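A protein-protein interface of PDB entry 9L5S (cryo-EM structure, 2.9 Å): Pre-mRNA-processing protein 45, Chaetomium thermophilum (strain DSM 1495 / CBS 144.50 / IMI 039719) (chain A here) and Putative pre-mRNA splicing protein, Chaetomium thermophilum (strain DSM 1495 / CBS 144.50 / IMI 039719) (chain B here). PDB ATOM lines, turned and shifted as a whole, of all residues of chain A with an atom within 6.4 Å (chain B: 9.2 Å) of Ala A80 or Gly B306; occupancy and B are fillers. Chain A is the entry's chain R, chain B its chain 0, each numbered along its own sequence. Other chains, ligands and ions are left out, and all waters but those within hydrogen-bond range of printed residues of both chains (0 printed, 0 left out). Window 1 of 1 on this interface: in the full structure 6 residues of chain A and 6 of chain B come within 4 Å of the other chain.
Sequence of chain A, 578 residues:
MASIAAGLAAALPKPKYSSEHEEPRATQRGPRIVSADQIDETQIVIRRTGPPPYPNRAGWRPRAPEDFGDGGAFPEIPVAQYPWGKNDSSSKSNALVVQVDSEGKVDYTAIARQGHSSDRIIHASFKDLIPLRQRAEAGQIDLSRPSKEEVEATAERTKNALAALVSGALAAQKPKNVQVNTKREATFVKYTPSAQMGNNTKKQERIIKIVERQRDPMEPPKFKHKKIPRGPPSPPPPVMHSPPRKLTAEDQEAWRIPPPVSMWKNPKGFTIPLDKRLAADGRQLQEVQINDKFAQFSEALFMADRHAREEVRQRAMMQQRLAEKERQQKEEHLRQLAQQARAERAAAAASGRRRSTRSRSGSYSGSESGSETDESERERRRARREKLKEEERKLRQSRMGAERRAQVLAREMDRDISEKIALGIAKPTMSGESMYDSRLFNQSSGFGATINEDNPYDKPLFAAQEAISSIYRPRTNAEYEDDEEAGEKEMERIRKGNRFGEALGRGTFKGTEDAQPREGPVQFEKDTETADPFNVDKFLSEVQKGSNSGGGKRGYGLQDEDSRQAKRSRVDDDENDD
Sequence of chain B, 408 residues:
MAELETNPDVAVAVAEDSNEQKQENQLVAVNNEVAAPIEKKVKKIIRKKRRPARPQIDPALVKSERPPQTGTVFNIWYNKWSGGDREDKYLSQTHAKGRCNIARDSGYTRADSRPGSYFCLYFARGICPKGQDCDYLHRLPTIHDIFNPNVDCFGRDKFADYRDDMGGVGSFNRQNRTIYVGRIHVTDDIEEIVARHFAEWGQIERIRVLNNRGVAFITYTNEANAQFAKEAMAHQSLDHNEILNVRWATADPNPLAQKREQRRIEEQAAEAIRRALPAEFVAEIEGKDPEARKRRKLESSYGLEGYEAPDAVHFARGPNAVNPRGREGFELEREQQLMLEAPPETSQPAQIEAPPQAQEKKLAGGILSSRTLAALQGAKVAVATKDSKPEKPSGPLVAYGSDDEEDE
Among the printed residues, merely in contact across the chains: Pro A78 with Leu B304, Val A79 with Glu B305, Ala A80 with Gly B306, Ala A80 with Glu B305, Val A79 with Leu B304 and Ala A80 with Leu B304.
The side-chain amide nitrogen (NE2) of Gln A81 sits at hydrogen-bond distance from the backbone carbonyl oxygen (O) of Val A79, at 2.5 Å.
O of Tyr B307 lies within hydrogen-bond range of OH of Tyr A82.
O of Pro A78 lies close to OE2 of Glu B305, at 3.0 Å.
Of the printed residues of chain A, Gly B306 touches Ala A80 (3.5 Å).
Val A79 touches just these residues of chain B: Leu B304 and Glu B305.
Of the printed residues of chain A, Tyr B307 touches Tyr A82 (3.4 Å).
Of the printed residues of chain A, Glu B305 touches Pro A78, Val A79 and Ala A80.
Printed residues of chain B within 4 Å of Tyr A82: Tyr B307 (3.4 Å).
Of the printed residues of chain B, Pro A78 touches Leu B304 (3.4 Å) and Glu B305 (3.0 Å).
Of the printed residues of chain A, Leu B304 touches Pro A78, Val A79 and Ala A80.
The nearest residue of chain B that does not touch Ala A80 is Tyr B307 (4.2 Å).
The nearest printed residue of chain B that does not touch Tyr A82 is Gly B306 (4.6 Å).
Of the 11 printed residues of chain B, 4 touch a printed residue of chain A.
Hydrophobic or aromatic side chains of chain B that line the printed part of chain A: Leu B304.
Along chain B the printed residues that touch a printed residue of chain A span positions 304 to 307.
Of the 6 printed residues of chain A, 4 touch a printed residue of chain B.
Among the printed residues, no Asp or Glu carboxylate lies within 4 Å of a Lys or Arg side-chain nitrogen of the other chain.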
ATOM      1  N   ILE A  77      13.654  -0.848  17.128  1.00  0.00           N
ATOM      2  CA  ILE A  77      14.669  -1.355  16.207  1.00  0.00           C
ATOM      3  C   ILE A  77      15.213  -2.678  16.733  1.00  0.00           C
ATOM      4  O   ILE A  77      15.750  -2.730  17.849  1.00  0.00           O
ATOM      5  CB  ILE A  77      15.805  -0.336  15.987  1.00  0.00           C
ATOM      6  CG1 ILE A  77      15.301   0.959  15.323  1.00  0.00           C
ATOM      7  CG2 ILE A  77      16.934  -0.954  15.187  1.00  0.00           C
ATOM      8  CD1 ILE A  77      14.816   2.055  16.258  1.00  0.00           C
ATOM      9  N   PRO A  78      15.100  -3.773  15.967  1.00  0.00           N
ATOM     10  CA  PRO A  78      15.642  -5.054  16.423  1.00  0.00           C
ATOM     11  C   PRO A  78      17.094  -5.269  16.026  1.00  0.00           C
ATOM     12  O   PRO A  78      17.455  -6.325  15.499  1.00  0.00           O
ATOM     13  CB  PRO A  78      14.702  -6.057  15.744  1.00  0.00           C
ATOM     14  CG  PRO A  78      14.224  -5.305  14.448  1.00  0.00           C
ATOM     15  CD  PRO A  78      14.768  -3.879  14.540  1.00  0.00           C
ATOM     16  N   VAL A  79      17.934  -4.269  16.284  1.00  0.00           N
ATOM     17  CA  VAL A  79      19.375  -4.351  16.084  1.00  0.00           C
ATOM     18  C   VAL A  79      20.033  -3.978  17.405  1.00  0.00           C
ATOM     19  O   VAL A  79      19.528  -3.124  18.142  1.00  0.00           O
ATOM     20  CB  VAL A  79      19.864  -3.429  14.935  1.00  0.00           C
ATOM     21  CG1 VAL A  79      21.342  -3.654  14.631  1.00  0.00           C
ATOM     22  CG2 VAL A  79      19.040  -3.644  13.674  1.00  0.00           C
ATOM     23  N   ALA A  80      21.136  -4.657  17.727  1.00  0.00           N
ATOM     24  CA  ALA A  80      21.895  -4.350  18.933  1.00  0.00           C
ATOM     25  C   ALA A  80      22.402  -2.914  18.900  1.00  0.00           C
ATOM     26  O   ALA A  80      23.014  -2.478  17.921  1.00  0.00           O
ATOM     27  CB  ALA A  80      23.067  -5.322  19.077  1.00  0.00           C
ATOM     28  N   GLN A  81      22.142  -2.182  19.980  1.00  0.00           N
ATOM     29  CA  GLN A  81      22.397  -0.752  20.047  1.00  0.00           C
ATOM     30  C   GLN A  81      23.245  -0.449  21.272  1.00  0.00           C
ATOM     31  O   GLN A  81      23.010  -1.003  22.349  1.00  0.00           O
ATOM     32  CB  GLN A  81      21.086   0.035  20.108  1.00  0.00           C
ATOM     33  CG  GLN A  81      20.305   0.059  18.808  1.00  0.00           C
ATOM     34  CD  GLN A  81      18.807   0.011  19.038  1.00  0.00           C
ATOM     35  OE1 GLN A  81      18.222   0.942  19.593  1.00  0.00           O
ATOM     36  NE2 GLN A  81      18.178  -1.078  18.614  1.00  0.00           N
ATOM     37  N   TYR A  82      24.224   0.435  21.104  1.00  0.00           N
ATOM     38  CA  TYR A  82      25.202   0.743  22.148  1.00  0.00           C
ATOM     39  C   TYR A  82      25.124   2.227  22.482  1.00  0.00           C
ATOM     40  O   TYR A  82      25.803   3.046  21.838  1.00  0.00           O
ATOM     41  CB  TYR A  82      26.615   0.367  21.696  1.00  0.00           C
ATOM     42  CG  TYR A  82      26.874  -1.125  21.549  1.00  0.00           C
ATOM     43  CD1 TYR A  82      26.013  -2.066  22.096  1.00  0.00           C
ATOM     44  CD2 TYR A  82      27.969  -1.587  20.830  1.00  0.00           C
ATOM     45  CE1 TYR A  82      26.242  -3.421  21.952  1.00  0.00           C
ATOM     46  CE2 TYR A  82      28.204  -2.944  20.679  1.00  0.00           C
ATOM     47  CZ  TYR A  82      27.339  -3.854  21.243  1.00  0.00           C
ATOM     48  OH  TYR A  82      27.570  -5.203  21.097  1.00  0.00           O
ATOM     49  N   LYS B 297      30.096 -17.553  16.295  1.00  0.00           N
ATOM     50  CA  LYS B 297      29.362 -16.497  15.593  1.00  0.00           C
ATOM     51  C   LYS B 297      27.867 -16.797  15.516  1.00  0.00           C
ATOM     52  O   LYS B 297      27.043 -15.897  15.713  1.00  0.00           O
ATOM     53  CB  LYS B 297      29.920 -16.262  14.184  1.00  0.00           C
ATOM     54  CG  LYS B 297      31.427 -16.041  14.057  1.00  0.00           C
ATOM     55  CD  LYS B 297      32.000 -15.169  15.169  1.00  0.00           C
ATOM     56  CE  LYS B 297      33.511 -15.304  15.245  1.00  0.00           C
ATOM     57  NZ  LYS B 297      33.914 -16.565  15.924  1.00  0.00           N
ATOM     58  N   SER B 300      26.257 -17.111  19.532  1.00  0.00           N
ATOM     59  CA  SER B 300      26.231 -15.886  20.333  1.00  0.00           C
ATOM     60  C   SER B 300      25.498 -14.756  19.616  1.00  0.00           C
ATOM     61  O   SER B 300      26.014 -13.650  19.455  1.00  0.00           O
ATOM     62  CB  SER B 300      27.652 -15.472  20.698  1.00  0.00           C
ATOM     63  OG  SER B 300      28.359 -15.017  19.558  1.00  0.00           O
ATOM     64  N   SER B 301      24.274 -15.038  19.177  1.00  0.00           N
ATOM     65  CA  SER B 301      23.392 -14.040  18.585  1.00  0.00           C
ATOM     66  C   SER B 301      22.103 -13.886  19.372  1.00  0.00           C
ATOM     67  O   SER B 301      21.695 -12.754  19.664  1.00  0.00           O
ATOM     68  CB  SER B 301      23.081 -14.409  17.125  1.00  0.00           C
ATOM     69  OG  SER B 301      24.266 -14.454  16.349  1.00  0.00           O
ATOM     70  N   TYR B 302      21.456 -15.005  19.719  1.00  0.00           N
ATOM     71  CA  TYR B 302      20.270 -15.051  20.581  1.00  0.00           C
ATOM     72  C   TYR B 302      19.112 -14.227  20.021  1.00  0.00           C
ATOM     73  O   TYR B 302      18.376 -13.581  20.770  1.00  0.00           O
ATOM     74  CB  TYR B 302      20.603 -14.607  22.009  1.00  0.00           C
ATOM     75  CG  TYR B 302      21.529 -15.542  22.752  1.00  0.00           C
ATOM     76  CD1 TYR B 302      21.048 -16.698  23.353  1.00  0.00           C
ATOM     77  CD2 TYR B 302      22.889 -15.269  22.850  1.00  0.00           C
ATOM     78  CE1 TYR B 302      21.894 -17.556  24.033  1.00  0.00           C
ATOM     79  CE2 TYR B 302      23.743 -16.120  23.528  1.00  0.00           C
ATOM     80  CZ  TYR B 302      23.240 -17.262  24.116  1.00  0.00           C
ATOM     81  OH  TYR B 302      24.086 -18.112  24.791  1.00  0.00           O
ATOM     82  N   GLY B 303      18.930 -14.251  18.703  1.00  0.00           N
ATOM     83  CA  GLY B 303      17.878 -13.473  18.077  1.00  0.00           C
ATOM     84  C   GLY B 303      18.331 -12.123  17.558  1.00  0.00           C
ATOM     85  O   GLY B 303      18.170 -11.832  16.369  1.00  0.00           O
ATOM     86  N   LEU B 304      18.883 -11.284  18.435  1.00  0.00           N
ATOM     87  CA  LEU B 304      19.406  -9.991  18.011  1.00  0.00           C
ATOM     88  C   LEU B 304      20.636 -10.160  17.131  1.00  0.00           C
ATOM     89  O   LEU B 304      21.626 -10.779  17.533  1.00  0.00           O
ATOM     90  CB  LEU B 304      19.747  -9.124  19.227  1.00  0.00           C
ATOM     91  CG  LEU B 304      18.691  -8.149  19.756  1.00  0.00           C
ATOM     92  CD1 LEU B 304      18.436  -7.093  18.704  1.00  0.00           C
ATOM     93  CD2 LEU B 304      17.390  -8.822  20.143  1.00  0.00           C
ATOM     94  N   GLU B 305      20.567  -9.603  15.926  1.00  0.00           N
ATOM     95  CA  GLU B 305      21.686  -9.668  15.002  1.00  0.00           C
ATOM     96  C   GLU B 305      22.708  -8.582  15.324  1.00  0.00           C
ATOM     97  O   GLU B 305      22.386  -7.529  15.881  1.00  0.00           O
ATOM     98  CB  GLU B 305      21.201  -9.534  13.555  1.00  0.00           C
ATOM     99  CG  GLU B 305      20.696  -8.150  13.173  1.00  0.00           C
ATOM    100  CD  GLU B 305      19.210  -7.966  13.428  1.00  0.00           C
ATOM    101  OE1 GLU B 305      18.626  -8.759  14.196  1.00  0.00           O
ATOM    102  OE2 GLU B 305      18.625  -7.022  12.857  1.00  0.00           O
ATOM    103  N   GLY B 306      23.957  -8.857  14.962  1.00  0.00           N
ATOM    104  CA  GLY B 306      25.034  -7.914  15.244  1.00  0.00           C
ATOM    105  C   GLY B 306      25.313  -7.736  16.717  1.00  0.00           C
ATOM    106  O   GLY B 306      25.680  -6.637  17.154  1.00  0.00           O
ATOM    107  N   TYR B 307      25.142  -8.798  17.504  1.00  0.00           N
ATOM    108  CA  TYR B 307      25.421  -8.740  18.935  1.00  0.00           C
ATOM    109  C   TYR B 307      26.877  -9.101  19.222  1.00  0.00           C
ATOM    110  O   TYR B 307      27.637  -8.265  19.722  1.00  0.00           O
ATOM    111  CB  TYR B 307      24.476  -9.682  19.693  1.00  0.00           C
ATOM    112  CG  TYR B 307      24.558  -9.611  21.212  1.00  0.00           C
ATOM    113  CD1 TYR B 307      24.058 -10.644  21.993  1.00  0.00           C
ATOM    114  CD2 TYR B 307      25.076  -8.493  21.864  1.00  0.00           C
ATOM    115  CE1 TYR B 307      24.122 -10.594  23.372  1.00  0.00           C
ATOM    116  CE2 TYR B 307      25.141  -8.434  23.241  1.00  0.00           C
ATOM    117  CZ  TYR B 307      24.658  -9.485  23.990  1.00  0.00           C
ATOM    118  OH  TYR B 307      24.714  -9.426  25.364  1.00  0.00           O
ATOM    119  N   GLU B 308      27.270 -10.335  18.888  1.00  0.00           N
ATOM    120  CA  GLU B 308      28.555 -10.928  19.268  1.00  0.00           C
ATOM    121  C   GLU B 308      28.771 -10.817  20.782  1.00  0.00           C
ATOM    122  O   GLU B 308      29.607 -10.054  21.272  1.00  0.00           O
ATOM    123  CB  GLU B 308      29.717 -10.309  18.479  1.00  0.00           C
ATOM    124  CG  GLU B 308      30.975 -11.161  18.483  1.00  0.00           C
ATOM    125  CD  GLU B 308      30.844 -12.395  17.611  1.00  0.00           C
ATOM    126  OE1 GLU B 308      30.063 -12.360  16.636  1.00  0.00           O
ATOM    127  OE2 GLU B 308      31.517 -13.404  17.908  1.00  0.00           O
ATOM    128  N   ALA B 309      27.939 -11.587  21.504  1.00  0.00           N
ATOM    129  CA  ALA B 309      27.791 -11.625  22.959  1.00  0.00           C
ATOM    130  C   ALA B 309      29.127 -11.664  23.693  1.00  0.00           C
ATOM    131  O   ALA B 309      30.059 -12.348  23.252  1.00  0.00           O
ATOM    132  CB  ALA B 309      26.949 -12.836  23.364  1.00  0.00           C
